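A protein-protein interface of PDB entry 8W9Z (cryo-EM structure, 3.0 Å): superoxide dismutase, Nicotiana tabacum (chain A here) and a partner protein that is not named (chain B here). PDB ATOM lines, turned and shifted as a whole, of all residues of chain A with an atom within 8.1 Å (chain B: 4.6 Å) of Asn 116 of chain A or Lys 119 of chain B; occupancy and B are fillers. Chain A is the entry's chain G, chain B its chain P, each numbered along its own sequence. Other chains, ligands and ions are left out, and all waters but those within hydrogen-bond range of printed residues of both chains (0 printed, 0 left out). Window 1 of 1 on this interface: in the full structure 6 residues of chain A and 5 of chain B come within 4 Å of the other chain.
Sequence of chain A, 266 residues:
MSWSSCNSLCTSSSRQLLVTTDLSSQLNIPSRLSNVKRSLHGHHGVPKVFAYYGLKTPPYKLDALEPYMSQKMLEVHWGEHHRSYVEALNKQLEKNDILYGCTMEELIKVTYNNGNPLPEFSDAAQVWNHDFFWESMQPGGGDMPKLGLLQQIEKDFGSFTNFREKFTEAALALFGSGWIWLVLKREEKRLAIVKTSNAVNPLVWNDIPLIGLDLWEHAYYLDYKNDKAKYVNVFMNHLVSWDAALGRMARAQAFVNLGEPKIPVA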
ATOM      1  N   VAL A 110     -32.015 -19.899  19.673  1.00  0.00           N
ATOM      2  CA  VAL A 110     -30.951 -20.880  19.495  1.00  0.00           C
ATOM      3  C   VAL A 110     -31.012 -21.544  18.125  1.00  0.00           C
ATOM      4  O   VAL A 110     -29.988 -22.048  17.645  1.00  0.00           O
ATOM      5  CB  VAL A 110     -30.987 -21.934  20.615  1.00  0.00           C
ATOM      6  CG1 VAL A 110     -32.070 -22.969  20.359  1.00  0.00           C
ATOM      7  CG2 VAL A 110     -29.627 -22.599  20.773  1.00  0.00           C
ATOM      8  N   THR A 111     -32.176 -21.554  17.476  1.00  0.00           N
ATOM      9  CA  THR A 111     -32.279 -22.073  16.119  1.00  0.00           C
ATOM     10  C   THR A 111     -32.031 -21.010  15.060  1.00  0.00           C
ATOM     11  O   THR A 111     -31.755 -21.359  13.907  1.00  0.00           O
ATOM     12  CB  THR A 111     -33.655 -22.703  15.892  1.00  0.00           C
ATOM     13  OG1 THR A 111     -34.679 -21.769  16.255  1.00  0.00           O
ATOM     14  CG2 THR A 111     -33.806 -23.965  16.723  1.00  0.00           C
ATOM     15  N   TYR A 112     -32.129 -19.727  15.416  1.00  0.00           N
ATOM     16  CA  TYR A 112     -31.763 -18.675  14.473  1.00  0.00           C
ATOM     17  C   TYR A 112     -30.266 -18.697  14.187  1.00  0.00           C
ATOM     18  O   TYR A 112     -29.844 -18.486  13.044  1.00  0.00           O
ATOM     19  CB  TYR A 112     -32.193 -17.314  15.015  1.00  0.00           C
ATOM     20  CG  TYR A 112     -31.924 -16.159  14.081  1.00  0.00           C
ATOM     21  CD1 TYR A 112     -32.696 -15.964  12.946  1.00  0.00           C
ATOM     22  CD2 TYR A 112     -30.907 -15.253  14.342  1.00  0.00           C
ATOM     23  CE1 TYR A 112     -32.458 -14.907  12.092  1.00  0.00           C
ATOM     24  CE2 TYR A 112     -30.660 -14.191  13.494  1.00  0.00           C
ATOM     25  CZ  TYR A 112     -31.439 -14.024  12.371  1.00  0.00           C
ATOM     26  OH  TYR A 112     -31.197 -12.968  11.524  1.00  0.00           O
ATOM     27  N   ASN A 113     -29.453 -18.949  15.215  1.00  0.00           N
ATOM     28  CA  ASN A 113     -28.008 -19.141  15.077  1.00  0.00           C
ATOM     29  C   ASN A 113     -27.322 -17.929  14.450  1.00  0.00           C
ATOM     30  O   ASN A 113     -26.287 -18.061  13.792  1.00  0.00           O
ATOM     31  CB  ASN A 113     -27.693 -20.412  14.281  1.00  0.00           C
ATOM     32  CG  ASN A 113     -26.284 -20.915  14.516  1.00  0.00           C
ATOM     33  OD1 ASN A 113     -25.636 -20.545  15.494  1.00  0.00           O
ATOM     34  ND2 ASN A 113     -25.801 -21.764  13.616  1.00  0.00           N
ATOM     35  N   ASN A 114     -27.899 -16.744  14.649  1.00  0.00           N
ATOM     36  CA  ASN A 114     -27.288 -15.475  14.252  1.00  0.00           C
ATOM     37  C   ASN A 114     -27.007 -15.436  12.747  1.00  0.00           C
ATOM     38  O   ASN A 114     -25.867 -15.292  12.300  1.00  0.00           O
ATOM     39  CB  ASN A 114     -26.015 -15.213  15.064  1.00  0.00           C
ATOM     40  CG  ASN A 114     -25.500 -13.799  14.900  1.00  0.00           C
ATOM     41  OD1 ASN A 114     -26.244 -12.896  14.518  1.00  0.00           O
ATOM     42  ND2 ASN A 114     -24.219 -13.598  15.189  1.00  0.00           N
ATOM     43  N   GLY A 115     -28.077 -15.573  11.966  1.00  0.00           N
ATOM     44  CA  GLY A 115     -28.020 -15.405  10.532  1.00  0.00           C
ATOM     45  C   GLY A 115     -28.011 -16.691   9.730  1.00  0.00           C
ATOM     46  O   GLY A 115     -28.394 -16.670   8.555  1.00  0.00           O
ATOM     47  N   ASN A 116     -27.580 -17.806  10.325  1.00  0.00           N
ATOM     48  CA  ASN A 116     -27.514 -19.102   9.651  1.00  0.00           C
ATOM     49  C   ASN A 116     -28.497 -20.040  10.342  1.00  0.00           C
ATOM     50  O   ASN A 116     -28.105 -20.848  11.198  1.00  0.00           O
ATOM     51  CB  ASN A 116     -26.093 -19.665   9.674  1.00  0.00           C
ATOM     52  CG  ASN A 116     -25.962 -20.951   8.883  1.00  0.00           C
ATOM     53  OD1 ASN A 116     -26.084 -22.046   9.433  1.00  0.00           O
ATOM     54  ND2 ASN A 116     -25.711 -20.825   7.586  1.00  0.00           N
ATOM     55  N   PRO A 117     -29.778 -19.968   9.991  1.00  0.00           N
ATOM     56  CA  PRO A 117     -30.795 -20.702  10.751  1.00  0.00           C
ATOM     57  C   PRO A 117     -30.662 -22.209  10.609  1.00  0.00           C
ATOM     58  O   PRO A 117     -30.280 -22.733   9.560  1.00  0.00           O
ATOM     59  CB  PRO A 117     -32.115 -20.208  10.145  1.00  0.00           C
ATOM     60  CG  PRO A 117     -31.771 -18.935   9.440  1.00  0.00           C
ATOM     61  CD  PRO A 117     -30.378 -19.129   8.943  1.00  0.00           C
ATOM     62  N   LEU A 118     -30.986 -22.905  11.696  1.00  0.00           N
ATOM     63  CA  LEU A 118     -31.052 -24.353  11.687  1.00  0.00           C
ATOM     64  C   LEU A 118     -32.297 -24.812  10.929  1.00  0.00           C
ATOM     65  O   LEU A 118     -33.232 -24.034  10.730  1.00  0.00           O
ATOM     66  CB  LEU A 118     -31.061 -24.884  13.119  1.00  0.00           C
ATOM     67  CG  LEU A 118     -29.812 -24.582  13.949  1.00  0.00           C
ATOM     68  CD1 LEU A 118     -29.885 -25.273  15.301  1.00  0.00           C
ATOM     69  CD2 LEU A 118     -28.557 -24.992  13.199  1.00  0.00           C
ATOM     70  N   PRO A 119     -32.334 -26.075  10.490  1.00  0.00           N
ATOM     71  CA  PRO A 119     -33.469 -26.533   9.670  1.00  0.00           C
ATOM     72  C   PRO A 119     -34.808 -26.543  10.391  1.00  0.00           C
ATOM     73  O   PRO A 119     -35.833 -26.760   9.734  1.00  0.00           O
ATOM     74  CB  PRO A 119     -33.056 -27.953   9.257  1.00  0.00           C
ATOM     75  CG  PRO A 119     -32.053 -28.367  10.276  1.00  0.00           C
ATOM     76  CD  PRO A 119     -31.304 -27.120  10.616  1.00  0.00           C
ATOM     77  N   PHE A 121     -35.735 -23.881  12.532  1.00  0.00           N
ATOM     78  CA  PHE A 121     -36.052 -22.528  12.978  1.00  0.00           C
ATOM     79  C   PHE A 121     -37.361 -22.040  12.377  1.00  0.00           C
ATOM     80  O   PHE A 121     -38.206 -21.473  13.080  1.00  0.00           O
ATOM     81  CB  PHE A 121     -34.918 -21.571  12.621  1.00  0.00           C
ATOM     82  CG  PHE A 121     -35.310 -20.123  12.698  1.00  0.00           C
ATOM     83  CD1 PHE A 121     -35.434 -19.492  13.921  1.00  0.00           C
ATOM     84  CD2 PHE A 121     -35.558 -19.396  11.547  1.00  0.00           C
ATOM     85  CE1 PHE A 121     -35.798 -18.161  13.996  1.00  0.00           C
ATOM     86  CE2 PHE A 121     -35.920 -18.067  11.616  1.00  0.00           C
ATOM     87  CZ  PHE A 121     -36.041 -17.449  12.841  1.00  0.00           C
ATOM     88  N   ASN B  49     -21.380 -25.282  14.844  1.00  0.00           N
ATOM     89  CA  ASN B  49     -22.504 -25.966  14.203  1.00  0.00           C
ATOM     90  C   ASN B  49     -21.989 -26.786  13.024  1.00  0.00           C
ATOM     91  O   ASN B  49     -22.132 -26.424  11.854  1.00  0.00           O
ATOM     92  CB  ASN B  49     -23.565 -24.964  13.767  1.00  0.00           C
ATOM     93  CG  ASN B  49     -24.813 -25.636  13.240  1.00  0.00           C
ATOM     94  OD1 ASN B  49     -25.061 -25.657  12.036  1.00  0.00           O
ATOM     95  ND2 ASN B  49     -25.603 -26.204  14.144  1.00  0.00           N
ATOM     96  N   HIS B  84     -17.495 -19.456   2.991  1.00  0.00           N
ATOM     97  CA  HIS B  84     -18.452 -18.438   2.589  1.00  0.00           C
ATOM     98  C   HIS B  84     -19.855 -18.985   2.377  1.00  0.00           C
ATOM     99  O   HIS B  84     -20.809 -18.203   2.387  1.00  0.00           O
ATOM    100  CB  HIS B  84     -17.994 -17.748   1.295  1.00  0.00           C
ATOM    101  CG  HIS B  84     -16.684 -17.036   1.416  1.00  0.00           C
ATOM    102  ND1 HIS B  84     -16.523 -15.900   2.179  1.00  0.00           N
ATOM    103  CD2 HIS B  84     -15.475 -17.292   0.862  1.00  0.00           C
ATOM    104  CE1 HIS B  84     -15.269 -15.489   2.095  1.00  0.00           C
ATOM    105  NE2 HIS B  84     -14.613 -16.316   1.302  1.00  0.00           N
ATOM    106  N   VAL B  85     -20.000 -20.293   2.182  1.00  0.00           N
ATOM    107  CA  VAL B  85     -21.287 -20.951   2.021  1.00  0.00           C
ATOM    108  C   VAL B  85     -21.226 -22.303   2.724  1.00  0.00           C
ATOM    109  O   VAL B  85     -20.180 -22.717   3.227  1.00  0.00           O
ATOM    110  CB  VAL B  85     -21.675 -21.131   0.538  1.00  0.00           C
ATOM    111  CG1 VAL B  85     -22.105 -19.807  -0.067  1.00  0.00           C
ATOM    112  CG2 VAL B  85     -20.515 -21.727  -0.244  1.00  0.00           C
ATOM    113  N   ASP B  86     -22.362 -22.992   2.756  1.00  0.00           N
ATOM    114  CA  ASP B  86     -22.407 -24.323   3.339  1.00  0.00           C
ATOM    115  C   ASP B  86     -21.641 -25.311   2.465  1.00  0.00           C
ATOM    116  O   ASP B  86     -21.342 -25.049   1.296  1.00  0.00           O
ATOM    117  CB  ASP B  86     -23.853 -24.785   3.515  1.00  0.00           C
ATOM    118  CG  ASP B  86     -24.657 -23.858   4.403  1.00  0.00           C
ATOM    119  OD1 ASP B  86     -24.939 -22.719   3.976  1.00  0.00           O
ATOM    120  OD2 ASP B  86     -25.008 -24.267   5.530  1.00  0.00           O
ATOM    121  N   TYR B 117     -20.156 -28.365   6.936  1.00  0.00           N
ATOM    122  CA  TYR B 117     -19.433 -27.232   7.499  1.00  0.00           C
ATOM    123  C   TYR B 117     -20.305 -25.983   7.444  1.00  0.00           C
ATOM    124  O   TYR B 117     -20.910 -25.702   6.404  1.00  0.00           O
ATOM    125  CB  TYR B 117     -18.126 -27.000   6.750  1.00  0.00           C
ATOM    126  CG  TYR B 117     -17.116 -28.105   6.950  1.00  0.00           C
ATOM    127  CD1 TYR B 117     -16.236 -28.080   8.022  1.00  0.00           C
ATOM    128  CD2 TYR B 117     -17.043 -29.174   6.068  1.00  0.00           C
ATOM    129  CE1 TYR B 117     -15.312 -29.087   8.210  1.00  0.00           C
ATOM    130  CE2 TYR B 117     -16.123 -30.186   6.249  1.00  0.00           C
ATOM    131  CZ  TYR B 117     -15.261 -30.137   7.321  1.00  0.00           C
ATOM    132  OH  TYR B 117     -14.342 -31.144   7.505  1.00  0.00           O
ATOM    133  N   PRO B 118     -20.395 -25.219   8.524  1.00  0.00           N
ATOM    134  CA  PRO B 118     -21.291 -24.063   8.563  1.00  0.00           C
ATOM    135  C   PRO B 118     -20.686 -22.865   7.838  1.00  0.00           C
ATOM    136  O   PRO B 118     -19.558 -22.895   7.352  1.00  0.00           O
ATOM    137  CB  PRO B 118     -21.431 -23.794  10.060  1.00  0.00           C
ATOM    138  CG  PRO B 118     -20.120 -24.220  10.618  1.00  0.00           C
ATOM    139  CD  PRO B 118     -19.702 -25.421   9.807  1.00  0.00           C
ATOM    140  N   LYS B 119     -21.472 -21.796   7.780  1.00  0.00           N
ATOM    141  CA  LYS B 119     -21.028 -20.541   7.196  1.00  0.00           C
ATOM    142  C   LYS B 119     -20.180 -19.768   8.199  1.00  0.00           C
ATOM    143  O   LYS B 119     -20.320 -19.930   9.414  1.00  0.00           O
ATOM    144  CB  LYS B 119     -22.235 -19.704   6.771  1.00  0.00           C
ATOM    145  CG  LYS B 119     -21.952 -18.628   5.736  1.00  0.00           C
ATOM    146  CD  LYS B 119     -23.198 -17.791   5.487  1.00  0.00           C
ATOM    147  CE  LYS B 119     -23.087 -16.973   4.212  1.00  0.00           C
ATOM    148  NZ  LYS B 119     -21.896 -16.082   4.209  1.00  0.00           N
ATOM    149  N   TRP B 120     -19.288 -18.927   7.675  1.00  0.00           N
ATOM    150  CA  TRP B 120     -18.420 -18.078   8.492  1.00  0.00           C
ATOM    151  C   TRP B 120     -17.539 -18.901   9.430  1.00  0.00           C
ATOM    152  O   TRP B 120     -17.203 -18.461  10.531  1.00  0.00           O
ATOM    153  CB  TRP B 120     -19.236 -17.053   9.286  1.00  0.00           C
ATOM    154  CG  TRP B 120     -20.108 -16.198   8.425  1.00  0.00           C
ATOM    155  CD1 TRP B 120     -19.779 -15.640   7.227  1.00  0.00           C
ATOM    156  CD2 TRP B 120     -21.464 -15.816   8.687  1.00  0.00           C
ATOM    157  NE1 TRP B 120     -20.841 -14.925   6.730  1.00  0.00           N
ATOM    158  CE2 TRP B 120     -21.888 -15.021   7.607  1.00  0.00           C
ATOM    159  CE3 TRP B 120     -22.358 -16.069   9.731  1.00  0.00           C
ATOM    160  CZ2 TRP B 120     -23.166 -14.474   7.542  1.00  0.00           C
ATOM    161  CZ3 TRP B 120     -23.625 -15.526   9.664  1.00  0.00           C
ATOM    162  CH2 TRP B 120     -24.018 -14.738   8.577  1.00  0.00           C
ATOM    163  N   PHE B 121     -17.162 -20.100   8.998  1.00  0.00           N
ATOM    164  CA  PHE B 121     -16.315 -20.984   9.784  1.00  0.00           C
ATOM    165  C   PHE B 121     -14.857 -20.770   9.397  1.00  0.00           C
ATOM    166  O   PHE B 121     -14.519 -20.756   8.210  1.00  0.00           O
ATOM    167  CB  PHE B 121     -16.722 -22.442   9.561  1.00  0.00           C
ATOM    168  CG  PHE B 121     -16.164 -23.404  10.575  1.00  0.00           C
ATOM    169  CD1 PHE B 121     -15.537 -22.952  11.723  1.00  0.00           C
ATOM    170  CD2 PHE B 121     -16.267 -24.769  10.371  1.00  0.00           C
ATOM    171  CE1 PHE B 121     -15.027 -23.842  12.646  1.00  0.00           C
ATOM    172  CE2 PHE B 121     -15.759 -25.663  11.290  1.00  0.00           C
ATOM    173  CZ  PHE B 121     -15.138 -25.200  12.427  1.00  0.00           C
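NZ of Lys 119 of chain B is in hydrogen-bond range of O of His 84 of chain B (3.0 Å).
The side-chain amide nitrogen (ND2) of Asn 113 of chain A lies close to the backbone carbonyl oxygen (O) of Asn 116 of chain A (3.5 Å).
The backbone NH (N) of Leu 118 of chain A is in hydrogen-bond range of the backbone carbonyl oxygen (O) of Thr 111 of chain A, at 2.8 Å.
Among the printed residues, pairs that only touch across the chains: Leu 118 of chain A with Asn 49 of chain B (3.3 Å), Asn 114 of chain A with Trp 120 of chain B (3.5 Å), Asn 116 of chain A with Lys 119 of chain B (3.7 Å) and Asn 113 of chain A with Asn 49 of chain B (3.9 Å).
Asn 116 of chain A touches one residue of chain B.
Of chain A, only Asn 116 comes within 4 Å of Lys 119 of chain B.
Of the printed residues of chain A, Trp 120 of chain B touches Asn 114 (3.5 Å).
Printed residues of chain B within 4 Å of Asn 114 of chain A: Trp 120.
Of the printed residues of chain A, Asn 49 of chain B touches Asn 113 (3.9 Å) and Leu 118 (3.3 Å).
Of the printed residues of chain B, Asn 113 of chain A touches Asn 49.
Printed residues of chain B within 4 Å of Leu 118 of chain A: Asn 49 (3.3 Å).
Gly 115 of chain A touches none of the printed residues of chain B.
Phe 121 of chain B touches none of the printed residues of chain A.
The nearest printed residue of chain A that does not touch Asn 49 of chain B is Asn 116 of chain A (4.6 Å).
Hydrophobic or aromatic side chains of chain B that line the printed part of chain A: Trp 120.
Along chain B the printed residues that touch a printed residue of chain A span positions 49 to 120.
Hydrophobic or aromatic side chains of chain A that line the printed part of chain B: Leu 118.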
